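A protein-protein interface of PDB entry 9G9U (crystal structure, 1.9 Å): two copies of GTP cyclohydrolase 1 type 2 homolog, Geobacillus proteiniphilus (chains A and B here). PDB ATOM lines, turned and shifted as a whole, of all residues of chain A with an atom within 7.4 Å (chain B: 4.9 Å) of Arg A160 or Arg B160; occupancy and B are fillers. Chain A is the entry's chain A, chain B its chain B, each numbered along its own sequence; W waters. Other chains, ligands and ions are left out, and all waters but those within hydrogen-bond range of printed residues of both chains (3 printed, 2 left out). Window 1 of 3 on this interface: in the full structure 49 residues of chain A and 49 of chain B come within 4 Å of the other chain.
NH2 of Arg A160 lies within salt-bridge range of OE2 of Glu B204 (3.7 Å). O of Ile A161 lies within hydrogen-bond range of N of Gln B262 (2.9 Å). The side-chain carboxylate (OE2) of Glu A201 is in hydrogen-bond range of the backbone NH (N) of Glu B204, at 2.8 Å. The backbone NH (N) of His A228 sits at hydrogen-bond distance from the side-chain carboxylate (OE1) of Glu B204. The backbone NH of Gln A262 sits at hydrogen-bond distance from the backbone carbonyl oxygen of Ile B161 (2.9 Å). O of Val B159 lies within hydrogen-bond range of N of Ile A264 (2.8 Å). The guanidinium group (NH2) of Arg A160 lies close to the guanidinium group (NH1) of Arg B160.
Among the printed residues, merely in contact across the chains: Phe A158 with Arg B160 (3.96 Å), Phe A158 with Val B263 (3.9 Å), Val A159 with Gln B262 (3.9 Å), Val A159 with Val B263 (3.5 Å), Arg A160 with Phe B261 (3.6 Å), Arg A160 with Gln B262 (3.3 Å), Arg A160 with Val B263 (3.9 Å), Ile A161 with Phe B261 (3.4 Å), Ala A162 with Phe B261 (3.8 Å), Val A225 with Phe B261 (3.7 Å), Gly A227 with Glu B204 (3.7 Å), Ile A260 with Ile B161 (3.9 Å), Ile A260 with Ala B162 (3.3 Å), Phe A261 with Arg B160 (3.6 Å), Phe A261 with Ile B161 (3.3 Å), Phe A261 with Ala B162 (3.9 Å), Phe A261 with Glu B204 (3.997 Å), Phe A261 with Val B225 (3.8 Å), Gln A262 with Val B159 (3.95 Å), Gln A262 with Arg B160 (3.2 Å), Val A263 with Phe B158 (3.8 Å), Val A263 with Val B159 (3.5 Å) and Ile A264 with Phe B158 (3.2 Å).
N of Ala A162 sits at hydrogen-bond distance from O of Leu A223, at 2.9 Å. The backbone NH (N) of Gly A227 lies within hydrogen-bond range of the backbone carbonyl oxygen (O) of Gly A200 (2.9 Å). The side-chain carboxylate (OE1) of Glu A201 is in hydrogen-bond range of a ring nitrogen (ND1) of His A228, 2.7 Å away. The guanidinium group (NH1) of Arg B160 is in salt-bridge range of the side-chain carboxylate (OE2) of Glu B204, at 3.9 Å. The backbone carbonyl oxygen (O) of Arg B160 is in hydrogen-bond range of the backbone NH (N) of Val B225 (2.8 Å). The backbone NH (N) of Ala B162 lies within hydrogen-bond range of the backbone carbonyl oxygen (O) of Leu B223 (2.9 Å).
Phe A158 touches Arg B160, but with the chains exchanged Arg A160 does not touch Phe B158 (4.1 Å). Val A159 touches Gln B262, and with the chains exchanged Gln A262 touches Val B159. Arg A160 touches Glu B204, but with the chains exchanged Glu A204 does not touch Arg B160 (4.05 Å). Arg A160 touches Gln B262, and with the chains exchanged Gln A262 touches Arg B160. Positions printed for both chains: 158, 159, 160, 161, 162, 204, 223, 224, 225, 261, 262 and 263. Of the 30 pairs that touch across the chains among the printed residues, 19 have their exchanged pair printed and touching as well.
Hydrophobic or aromatic side chains of chain A that line the printed part of chain B: Phe A158, Ile A161, Ala A162, Val A225, His A228, Phe A261, Val A263 and Ile A264. Hydrophobic or aromatic side chains of chain B that line the printed part of chain A: Phe B158, Val B159, Ile B161, Ala B162, Val B225, Phe B261 and Val B263. Along chain B the printed residues that touch a printed residue of chain A span positions 158 to 263. Among the printed residues, 30 pairs touch across the chains.
Arg A160 touches just these residues of chain B: Arg B160, Glu B204, Phe B261, Gln B262 and Val B263. Printed residues of chain A within 4 Å of Phe B261: Arg A160, Ile A161, Ala A162 and Val A225. Of the printed residues of chain B, Glu A201 touches Glu B204. Of the printed residues of chain B, Gln A262 touches Val B159, Arg B160 and Ile B161. Ile A197 touches none of the printed residues of chain B. Ile B224 touches none of the printed residues of chain A. The nearest residue of chain B that does not touch Arg A160 is Phe B158 (4.1 Å). The nearest residue of chain A that does not touch Arg B160 is Glu A204 (4.05 Å).
Water W3 bridges OE2 of Glu A204 (2.5 Å) and NH2 of Arg B160 (2.8 Å). Water W2 lies within hydrogen-bond range of the side-chain carboxylate (OE2) of Glu B204 (2.6 Å), the guanidinium group (NH2) of Arg A160 (2.6 Å) and the backbone carbonyl oxygen (O) of Gly A200 (2.8 Å). Water W1 lies within hydrogen-bond range of NE2 of Gln A262 and O of Ile B161.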
ATOM      1  N   ALA A 147       2.691  22.769  20.092  1.00  0.00           N
ATOM      2  CA  ALA A 147       1.318  22.935  19.621  1.00  0.00           C
ATOM      3  C   ALA A 147       1.138  22.308  18.243  1.00  0.00           C
ATOM      4  O   ALA A 147       0.137  21.627  17.992  1.00  0.00           O
ATOM      5  CB  ALA A 147       0.957  24.422  19.622  1.00  0.00           C
ATOM      6  N   PHE A 158      -7.208  22.728  14.391  1.00  0.00           N
ATOM      7  CA  PHE A 158      -6.610  23.920  14.965  1.00  0.00           C
ATOM      8  C   PHE A 158      -6.369  23.670  16.442  1.00  0.00           C
ATOM      9  O   PHE A 158      -6.968  22.782  17.052  1.00  0.00           O
ATOM     10  CB  PHE A 158      -7.495  25.160  14.740  1.00  0.00           C
ATOM     11  CG  PHE A 158      -8.771  25.172  15.557  1.00  0.00           C
ATOM     12  CD1 PHE A 158      -9.933  24.601  15.057  1.00  0.00           C
ATOM     13  CD2 PHE A 158      -8.804  25.767  16.813  1.00  0.00           C
ATOM     14  CE1 PHE A 158     -11.116  24.607  15.803  1.00  0.00           C
ATOM     15  CE2 PHE A 158      -9.973  25.777  17.567  1.00  0.00           C
ATOM     16  CZ  PHE A 158     -11.138  25.200  17.055  1.00  0.00           C
ATOM     17  N   VAL A 159      -5.455  24.448  17.008  1.00  0.00           N
ATOM     18  CA  VAL A 159      -5.284  24.492  18.448  1.00  0.00           C
ATOM     19  C   VAL A 159      -5.170  25.960  18.795  1.00  0.00           C
ATOM     20  O   VAL A 159      -4.932  26.807  17.927  1.00  0.00           O
ATOM     21  CB  VAL A 159      -4.047  23.712  18.935  1.00  0.00           C
ATOM     22  CG1 VAL A 159      -4.247  22.209  18.670  1.00  0.00           C
ATOM     23  CG2 VAL A 159      -2.818  24.229  18.256  1.00  0.00           C
ATOM     24  N   ARG A 160      -5.355  26.266  20.076  1.00  0.00           N
ATOM     25  CA  ARG A 160      -5.185  27.630  20.545  1.00  0.00           C
ATOM     26  C   ARG A 160      -4.013  27.654  21.508  1.00  0.00           C
ATOM     27  O   ARG A 160      -3.770  26.670  22.223  1.00  0.00           O
ATOM     28  CB  ARG A 160      -6.470  28.161  21.220  1.00  0.00           C
ATOM     29  CG  ARG A 160      -7.614  28.407  20.206  1.00  0.00           C
ATOM     30  CD  ARG A 160      -8.969  28.632  20.890  1.00  0.00           C
ATOM     31  NE  ARG A 160      -9.423  27.438  21.589  1.00  0.00           N
ATOM     32  CZ  ARG A 160     -10.233  27.452  22.649  1.00  0.00           C
ATOM     33  NH1 ARG A 160     -10.695  28.596  23.108  1.00  0.00           N
ATOM     34  NH2 ARG A 160     -10.589  26.319  23.235  1.00  0.00           N
ATOM     35  N   ILE A 161      -3.282  28.769  21.522  1.00  0.00           N
ATOM     36  CA  ILE A 161      -2.112  28.897  22.379  1.00  0.00           C
ATOM     37  C   ILE A 161      -2.128  30.284  23.019  1.00  0.00           C
ATOM     38  O   ILE A 161      -2.287  31.301  22.328  1.00  0.00           O
ATOM     39  CB  ILE A 161      -0.797  28.631  21.605  1.00  0.00           C
ATOM     40  CG1 ILE A 161       0.430  28.825  22.512  1.00  0.00           C
ATOM     41  CG2 ILE A 161      -0.662  29.566  20.399  1.00  0.00           C
ATOM     42  CD1 ILE A 161       1.665  28.024  22.056  1.00  0.00           C
ATOM     43  N   ALA A 162      -2.013  30.312  24.353  1.00  0.00           N
ATOM     44  CA  ALA A 162      -1.764  31.515  25.135  1.00  0.00           C
ATOM     45  C   ALA A 162      -0.297  31.616  25.541  1.00  0.00           C
ATOM     46  O   ALA A 162       0.399  30.609  25.680  1.00  0.00           O
ATOM     47  CB  ALA A 162      -2.625  31.541  26.392  1.00  0.00           C
ATOM     48  N   ILE A 197       1.664  24.031  29.733  1.00  0.00           N
ATOM     49  CA  ILE A 197       0.645  23.043  30.031  1.00  0.00           C
ATOM     50  C   ILE A 197      -0.213  22.871  28.789  1.00  0.00           C
ATOM     51  O   ILE A 197      -0.426  23.827  28.038  1.00  0.00           O
ATOM     52  CB  ILE A 197      -0.218  23.441  31.242  1.00  0.00           C
ATOM     53  CG1 ILE A 197       0.524  23.088  32.540  1.00  0.00           C
ATOM     54  CG2 ILE A 197      -1.533  22.698  31.211  1.00  0.00           C
ATOM     55  CD1 ILE A 197      -0.198  23.497  33.795  1.00  0.00           C
ATOM     56  N   TYR A 199      -3.947  21.436  27.745  1.00  0.00           N
ATOM     57  CA  TYR A 199      -5.182  20.951  28.321  1.00  0.00           C
ATOM     58  C   TYR A 199      -6.317  21.034  27.319  1.00  0.00           C
ATOM     59  O   TYR A 199      -6.184  21.568  26.219  1.00  0.00           O
ATOM     60  CB  TYR A 199      -5.526  21.692  29.634  1.00  0.00           C
ATOM     61  CG  TYR A 199      -5.959  23.154  29.650  1.00  0.00           C
ATOM     62  CD1 TYR A 199      -7.078  23.622  28.945  1.00  0.00           C
ATOM     63  CD2 TYR A 199      -5.310  24.042  30.484  1.00  0.00           C
ATOM     64  CE1 TYR A 199      -7.488  24.951  29.049  1.00  0.00           C
ATOM     65  CE2 TYR A 199      -5.714  25.369  30.600  1.00  0.00           C
ATOM     66  CZ  TYR A 199      -6.798  25.820  29.873  1.00  0.00           C
ATOM     67  OH  TYR A 199      -7.212  27.118  29.993  1.00  0.00           O
ATOM     68  N   GLY A 200      -7.422  20.414  27.710  1.00  0.00           N
ATOM     69  CA  GLY A 200      -8.552  20.275  26.802  1.00  0.00           C
ATOM     70  C   GLY A 200      -9.435  21.500  26.851  1.00  0.00           C
ATOM     71  O   GLY A 200      -9.614  22.193  25.843  1.00  0.00           O
ATOM     72  N   GLU A 201      -9.953  21.816  28.033  1.00  0.00           N
ATOM     73  CA  GLU A 201     -10.877  22.937  28.176  1.00  0.00           C
ATOM     74  C   GLU A 201     -10.759  23.501  29.586  1.00  0.00           C
ATOM     75  O   GLU A 201     -10.518  22.749  30.539  1.00  0.00           O
ATOM     76  CB  GLU A 201     -12.308  22.478  27.907  1.00  0.00           C
ATOM     77  CG  GLU A 201     -13.360  23.607  27.896  1.00  0.00           C
ATOM     78  CD  GLU A 201     -14.790  23.066  27.707  1.00  0.00           C
ATOM     79  OE1 GLU A 201     -14.976  21.831  27.643  1.00  0.00           O
ATOM     80  OE2 GLU A 201     -15.722  23.891  27.611  1.00  0.00           O
ATOM     81  N   GLY A 202     -10.905  24.822  29.716  1.00  0.00           N
ATOM     82  CA  GLY A 202     -10.990  25.447  31.012  1.00  0.00           C
ATOM     83  C   GLY A 202     -11.423  26.895  30.925  1.00  0.00           C
ATOM     84  O   GLY A 202     -11.449  27.493  29.854  1.00  0.00           O
ATOM     85  N   GLU A 204     -11.646  30.679  30.516  1.00  0.00           N
ATOM     86  CA  GLU A 204     -10.704  31.593  29.884  1.00  0.00           C
ATOM     87  C   GLU A 204     -10.106  32.591  30.864  1.00  0.00           C
ATOM     88  O   GLU A 204      -9.026  33.122  30.596  1.00  0.00           O
ATOM     89  CB  GLU A 204     -11.388  32.359  28.733  1.00  0.00           C
ATOM     90  CG  GLU A 204     -11.684  31.416  27.590  1.00  0.00           C
ATOM     91  CD  GLU A 204     -12.289  32.075  26.370  1.00  0.00           C
ATOM     92  OE1 GLU A 204     -12.176  33.302  26.230  1.00  0.00           O
ATOM     93  OE2 GLU A 204     -12.863  31.328  25.541  1.00  0.00           O
ATOM     94  N   LEU A 223       0.544  28.075  27.149  1.00  0.00           N
ATOM     95  CA  LEU A 223      -0.581  27.203  27.403  1.00  0.00           C
ATOM     96  C   LEU A 223      -1.128  26.767  26.052  1.00  0.00           C
ATOM     97  O   LEU A 223      -1.375  27.612  25.189  1.00  0.00           O
ATOM     98  CB  LEU A 223      -1.650  27.953  28.222  1.00  0.00           C
ATOM     99  CG  LEU A 223      -2.889  27.215  28.703  1.00  0.00           C
ATOM    100  CD1 LEU A 223      -2.562  26.104  29.717  1.00  0.00           C
ATOM    101  CD2 LEU A 223      -3.864  28.251  29.290  1.00  0.00           C
ATOM    102  N   ILE A 224      -1.262  25.459  25.850  1.00  0.00           N
ATOM    103  CA  ILE A 224      -1.820  24.917  24.619  1.00  0.00           C
ATOM    104  C   ILE A 224      -3.181  24.315  24.941  1.00  0.00           C
ATOM    105  O   ILE A 224      -3.288  23.377  25.742  1.00  0.00           O
ATOM    106  CB  ILE A 224      -0.896  23.875  23.986  1.00  0.00           C
ATOM    107  CG1 ILE A 224       0.450  24.506  23.620  1.00  0.00           C
ATOM    108  CG2 ILE A 224      -1.573  23.220  22.767  1.00  0.00           C
ATOM    109  CD1 ILE A 224       1.584  23.492  23.670  1.00  0.00           C
ATOM    110  N   VAL A 225      -4.216  24.831  24.285  1.00  0.00           N
ATOM    111  CA  VAL A 225      -5.596  24.432  24.527  1.00  0.00           C
ATOM    112  C   VAL A 225      -6.093  23.667  23.304  1.00  0.00           C
ATOM    113  O   VAL A 225      -6.167  24.221  22.195  1.00  0.00           O
ATOM    114  CB  VAL A 225      -6.476  25.661  24.812  1.00  0.00           C
ATOM    115  CG1 VAL A 225      -7.897  25.250  25.125  1.00  0.00           C
ATOM    116  CG2 VAL A 225      -5.874  26.425  26.004  1.00  0.00           C
ATOM    117  N   LEU A 226      -6.464  22.406  23.514  1.00  0.00           N
ATOM    118  CA  LEU A 226      -6.753  21.486  22.425  1.00  0.00           C
ATOM    119  C   LEU A 226      -8.225  21.421  22.052  1.00  0.00           C
ATOM    120  O   LEU A 226      -8.552  21.098  20.901  1.00  0.00           O
ATOM    121  CB  LEU A 226      -6.314  20.081  22.800  1.00  0.00           C
ATOM    122  CG  LEU A 226      -4.846  19.815  23.113  1.00  0.00           C
ATOM    123  CD1 LEU A 226      -4.750  18.358  23.580  1.00  0.00           C
ATOM    124  CD2 LEU A 226      -4.024  20.058  21.860  1.00  0.00           C
ATOM    125  N   GLY A 227      -9.113  21.669  22.993  1.00  0.00           N
ATOM    126  CA  GLY A 227     -10.498  21.263  22.801  1.00  0.00           C
ATOM    127  C   GLY A 227     -10.849  20.131  23.757  1.00  0.00           C
ATOM    128  O   GLY A 227     -10.022  19.274  24.072  1.00  0.00           O
ATOM    129  N   HIS A 228     -12.080  20.158  24.275  1.00  0.00           N
ATOM    130  CA  HIS A 228     -12.470  19.128  25.238  1.00  0.00           C
ATOM    131  C   HIS A 228     -12.503  17.755  24.582  1.00  0.00           C
ATOM    132  O   HIS A 228     -11.810  16.825  25.023  1.00  0.00           O
ATOM    133  CB  HIS A 228     -13.828  19.500  25.866  1.00  0.00           C
ATOM    134  CG  HIS A 228     -14.211  18.678  27.070  1.00  0.00           C
ATOM    135  ND1 HIS A 228     -14.932  19.201  28.125  1.00  0.00           N
ATOM    136  CD2 HIS A 228     -14.009  17.372  27.368  1.00  0.00           C
ATOM    137  CE1 HIS A 228     -15.173  18.249  29.009  1.00  0.00           C
ATOM    138  NE2 HIS A 228     -14.611  17.132  28.581  1.00  0.00           N
ATOM    139  N   ILE A 260     -16.168  19.991  16.744  1.00  0.00           N
ATOM    140  CA  ILE A 260     -17.403  20.709  17.048  1.00  0.00           C
ATOM    141  C   ILE A 260     -17.363  22.115  16.453  1.00  0.00           C
ATOM    142  O   ILE A 260     -18.393  22.663  16.034  1.00  0.00           O
ATOM    143  CB  ILE A 260     -17.644  20.742  18.568  1.00  0.00           C
ATOM    144  CG1 ILE A 260     -19.035  21.297  18.860  1.00  0.00           C
ATOM    145  CG2 ILE A 260     -16.614  21.617  19.307  1.00  0.00           C
ATOM    146  CD1 ILE A 260     -20.153  20.439  18.278  1.00  0.00           C
ATOM    147  N   PHE A 261     -16.173  22.712  16.360  1.00  0.00           N
ATOM    148  CA  PHE A 261     -16.047  24.091  15.902  1.00  0.00           C
ATOM    149  C   PHE A 261     -15.232  24.160  14.621  1.00  0.00           C
ATOM    150  O   PHE A 261     -14.300  23.378  14.407  1.00  0.00           O
ATOM    151  CB  PHE A 261     -15.362  24.995  16.952  1.00  0.00           C
ATOM    152  CG  PHE A 261     -16.157  25.211  18.204  1.00  0.00           C
ATOM    153  CD1 PHE A 261     -17.420  25.771  18.160  1.00  0.00           C
ATOM    154  CD2 PHE A 261     -15.611  24.890  19.439  1.00  0.00           C
ATOM    155  CE1 PHE A 261     -18.154  25.982  19.320  1.00  0.00           C
ATOM    156  CE2 PHE A 261     -16.329  25.106  20.618  1.00  0.00           C
ATOM    157  CZ  PHE A 261     -17.601  25.661  20.564  1.00  0.00           C
ATOM    158  N   GLN A 262     -15.563  25.151  13.796  1.00  0.00           N
ATOM    159  CA  GLN A 262     -14.678  25.625  12.745  1.00  0.00           C
ATOM    160  C   GLN A 262     -14.215  27.017  13.141  1.00  0.00           C
ATOM    161  O   GLN A 262     -14.936  27.741  13.832  1.00  0.00           O
ATOM    162  CB  GLN A 262     -15.367  25.642  11.378  1.00  0.00           C
ATOM    163  CG  GLN A 262     -15.901  24.262  10.978  1.00  0.00           C
ATOM    164  CD  GLN A 262     -16.535  24.221   9.594  1.00  0.00           C
ATOM    165  OE1 GLN A 262     -15.902  24.578   8.596  1.00  0.00           O
ATOM    166  NE2 GLN A 262     -17.787  23.772   9.530  1.00  0.00           N
ATOM    167  N   VAL A 263     -12.988  27.355  12.765  1.00  0.00           N
ATOM    168  CA  VAL A 263     -12.439  28.677  13.030  1.00  0.00           C
ATOM    169  C   VAL A 263     -12.684  29.553  11.815  1.00  0.00           C
ATOM    170  O   VAL A 263     -12.409  29.145  10.676  1.00  0.00           O
ATOM    171  CB  VAL A 263     -10.940  28.612  13.344  1.00  0.00           C
ATOM    172  CG1 VAL A 263     -10.419  30.004  13.618  1.00  0.00           C
ATOM    173  CG2 VAL A 263     -10.725  27.770  14.546  1.00  0.00           C
ATOM    174  N   ILE A 264     -13.238  30.740  12.061  1.00  0.00           N
ATOM    175  CA  ILE A 264     -13.351  31.807  11.073  1.00  0.00           C
ATOM    176  C   ILE A 264     -12.220  32.791  11.348  1.00  0.00           C
ATOM    177  O   ILE A 264     -12.205  33.443  12.398  1.00  0.00           O
ATOM    178  CB  ILE A 264     -14.713  32.512  11.165  1.00  0.00           C
ATOM    179  CG1 ILE A 264     -15.866  31.504  11.078  1.00  0.00           C
ATOM    180  CG2 ILE A 264     -14.842  33.593  10.087  1.00  0.00           C
ATOM    181  CD1 ILE A 264     -15.887  30.730   9.780  1.00  0.00           C
ATOM    182  N   PHE B 158     -10.138  35.904  15.454  1.00  0.00           N
ATOM    183  CA  PHE B 158     -10.873  34.735  14.989  1.00  0.00           C
ATOM    184  C   PHE B 158     -12.127  34.583  15.832  1.00  0.00           C
ATOM    185  O   PHE B 158     -12.216  35.097  16.949  1.00  0.00           O
ATOM    186  CB  PHE B 158     -10.040  33.455  15.081  1.00  0.00           C
ATOM    187  CG  PHE B 158      -9.737  33.040  16.498  1.00  0.00           C
ATOM    188  CD1 PHE B 158      -8.672  33.619  17.194  1.00  0.00           C
ATOM    189  CD2 PHE B 158     -10.544  32.130  17.164  1.00  0.00           C
ATOM    190  CE1 PHE B 158      -8.409  33.262  18.517  1.00  0.00           C
ATOM    191  CE2 PHE B 158     -10.289  31.774  18.483  1.00  0.00           C
ATOM    192  CZ  PHE B 158      -9.210  32.342  19.158  1.00  0.00           C
ATOM    193  N   VAL B 159     -13.093  33.847  15.287  1.00  0.00           N
ATOM    194  CA  VAL B 159     -14.233  33.379  16.059  1.00  0.00           C
ATOM    195  C   VAL B 159     -14.410  31.918  15.696  1.00  0.00           C
ATOM    196  O   VAL B 159     -13.812  31.418  14.739  1.00  0.00           O
ATOM    197  CB  VAL B 159     -15.535  34.153  15.768  1.00  0.00           C
ATOM    198  CG1 VAL B 159     -15.378  35.597  16.237  1.00  0.00           C
ATOM    199  CG2 VAL B 159     -15.914  34.025  14.291  1.00  0.00           C
ATOM    200  N   ARG B 160     -15.225  31.228  16.486  1.00  0.00           N
ATOM    201  CA  ARG B 160     -15.522  29.824  16.239  1.00  0.00           C
ATOM    202  C   ARG B 160     -17.014  29.652  15.988  1.00  0.00           C
ATOM    203  O   ARG B 160     -17.836  30.391  16.550  1.00  0.00           O
ATOM    204  CB  ARG B 160     -15.082  28.947  17.422  1.00  0.00           C
ATOM    205  CG  ARG B 160     -13.542  28.829  17.554  1.00  0.00           C
ATOM    206  CD  ARG B 160     -13.113  28.115  18.859  1.00  0.00           C
ATOM    207  NE  ARG B 160     -13.455  28.908  20.046  1.00  0.00           N
ATOM    208  CZ  ARG B 160     -13.630  28.406  21.272  1.00  0.00           C
ATOM    209  NH1 ARG B 160     -13.437  27.127  21.514  1.00  0.00           N
ATOM    210  NH2 ARG B 160     -13.965  29.215  22.270  1.00  0.00           N
ATOM    211  N   ILE B 161     -17.360  28.671  15.147  1.00  0.00           N
ATOM    212  CA  ILE B 161     -18.744  28.448  14.748  1.00  0.00           C
ATOM    213  C   ILE B 161     -19.015  26.948  14.794  1.00  0.00           C
ATOM    214  O   ILE B 161     -18.189  26.142  14.344  1.00  0.00           O
ATOM    215  CB  ILE B 161     -19.043  29.039  13.351  1.00  0.00           C
ATOM    216  CG1 ILE B 161     -20.522  28.889  12.966  1.00  0.00           C
ATOM    217  CG2 ILE B 161     -18.163  28.447  12.278  1.00  0.00           C
ATOM    218  CD1 ILE B 161     -20.927  29.898  11.879  1.00  0.00           C
ATOM    219  N   ALA B 162     -20.118  26.579  15.435  1.00  0.00           N
ATOM    220  CA  ALA B 162     -20.648  25.225  15.430  1.00  0.00           C
ATOM    221  C   ALA B 162     -21.949  25.208  14.643  1.00  0.00           C
ATOM    222  O   ALA B 162     -22.650  26.218  14.551  1.00  0.00           O
ATOM    223  CB  ALA B 162     -20.893  24.708  16.858  1.00  0.00           C
ATOM    224  N   GLU B 204     -18.117  23.312  26.357  1.00  0.00           N
ATOM    225  CA  GLU B 204     -18.111  22.777  25.001  1.00  0.00           C
ATOM    226  C   GLU B 204     -19.051  21.596  24.849  1.00  0.00           C
ATOM    227  O   GLU B 204     -19.467  21.285  23.720  1.00  0.00           O
ATOM    228  CB  GLU B 204     -16.673  22.351  24.584  1.00  0.00           C
ATOM    229  CG  GLU B 204     -15.746  23.533  24.246  1.00  0.00           C
ATOM    230  CD  GLU B 204     -14.316  23.127  23.845  1.00  0.00           C
ATOM    231  OE1 GLU B 204     -14.064  21.939  23.523  1.00  0.00           O
ATOM    232  OE2 GLU B 204     -13.454  24.032  23.841  1.00  0.00           O
ATOM    233  N   LEU B 223     -24.115  28.233  16.062  1.00  0.00           N
ATOM    234  CA  LEU B 223     -23.640  28.844  17.287  1.00  0.00           C
ATOM    235  C   LEU B 223     -22.333  29.567  16.993  1.00  0.00           C
ATOM    236  O   LEU B 223     -21.425  28.982  16.391  1.00  0.00           O
ATOM    237  CB  LEU B 223     -23.450  27.771  18.368  1.00  0.00           C
ATOM    238  CG  LEU B 223     -23.219  28.142  19.837  1.00  0.00           C
ATOM    239  CD1 LEU B 223     -24.501  28.756  20.462  1.00  0.00           C
ATOM    240  CD2 LEU B 223     -22.754  26.888  20.613  1.00  0.00           C
ATOM    241  N   ILE B 224     -22.248  30.834  17.399  1.00  0.00           N
ATOM    242  CA  ILE B 224     -21.067  31.650  17.160  1.00  0.00           C
ATOM    243  C   ILE B 224     -20.466  32.019  18.513  1.00  0.00           C
ATOM    244  O   ILE B 224     -21.114  32.664  19.352  1.00  0.00           O
ATOM    245  CB  ILE B 224     -21.387  32.899  16.327  1.00  0.00           C
ATOM    246  CG1 ILE B 224     -21.846  32.489  14.929  1.00  0.00           C
ATOM    247  CG2 ILE B 224     -20.181  33.810  16.228  1.00  0.00           C
ATOM    248  CD1 ILE B 224     -22.928  33.390  14.426  1.00  0.00           C
ATOM    249  N   VAL B 225     -19.220  31.608  18.719  1.00  0.00           N
ATOM    250  CA  VAL B 225     -18.550  31.701  20.009  1.00  0.00           C
ATOM    251  C   VAL B 225     -17.376  32.651  19.859  1.00  0.00           C
ATOM    252  O   VAL B 225     -16.424  32.363  19.124  1.00  0.00           O
ATOM    253  CB  VAL B 225     -18.076  30.318  20.475  1.00  0.00           C
ATOM    254  CG1 VAL B 225     -17.317  30.433  21.795  1.00  0.00           C
ATOM    255  CG2 VAL B 225     -19.275  29.389  20.552  1.00  0.00           C
ATOM    256  N   PHE B 261      -5.769  34.102  23.174  1.00  0.00           N
ATOM    257  CA  PHE B 261      -5.288  32.983  22.372  1.00  0.00           C
ATOM    258  C   PHE B 261      -4.880  33.434  20.977  1.00  0.00           C
ATOM    259  O   PHE B 261      -5.449  34.374  20.412  1.00  0.00           O
ATOM    260  CB  PHE B 261      -6.340  31.875  22.217  1.00  0.00           C
ATOM    261  CG  PHE B 261      -6.740  31.239  23.495  1.00  0.00           C
ATOM    262  CD1 PHE B 261      -5.791  30.654  24.323  1.00  0.00           C
ATOM    263  CD2 PHE B 261      -8.076  31.199  23.874  1.00  0.00           C
ATOM    264  CE1 PHE B 261      -6.182  30.045  25.522  1.00  0.00           C
ATOM    265  CE2 PHE B 261      -8.458  30.595  25.075  1.00  0.00           C
ATOM    266  CZ  PHE B 261      -7.500  30.036  25.897  1.00  0.00           C
ATOM    267  N   GLN B 262      -3.888  32.733  20.433  1.00  0.00           N
ATOM    268  CA  GLN B 262      -3.603  32.708  19.010  1.00  0.00           C
ATOM    269  C   GLN B 262      -4.049  31.353  18.472  1.00  0.00           C
ATOM    270  O   GLN B 262      -3.955  30.340  19.176  1.00  0.00           O
ATOM    271  CB  GLN B 262      -2.122  32.933  18.745  1.00  0.00           C
ATOM    272  CG  GLN B 262      -1.638  34.345  19.103  1.00  0.00           C
ATOM    273  CD  GLN B 262      -0.181  34.575  18.761  1.00  0.00           C
ATOM    274  OE1 GLN B 262       0.201  34.560  17.593  1.00  0.00           O
ATOM    275  NE2 GLN B 262       0.643  34.779  19.782  1.00  0.00           N
ATOM    276  N   VAL B 263      -4.552  31.316  17.238  1.00  0.00           N
ATOM    277  CA  VAL B 263      -4.937  30.037  16.643  1.00  0.00           C
ATOM    278  C   VAL B 263      -3.797  29.520  15.776  1.00  0.00           C
ATOM    279  O   VAL B 263      -3.183  30.269  15.001  1.00  0.00           O
ATOM    280  CB  VAL B 263      -6.229  30.155  15.826  1.00  0.00           C
ATOM    281  CG1 VAL B 263      -6.425  28.890  15.000  1.00  0.00           C
ATOM    282  CG2 VAL B 263      -7.394  30.300  16.773  1.00  0.00           C
HETATM  283  O   HOH W   1     -19.167  23.882  12.072  1.00  0.00           O
HETATM  284  O   HOH W   2     -11.145  24.383  24.904  1.00  0.00           O
HETATM  285  O   HOH W   3     -14.989  30.867  24.342  1.00  0.00           O
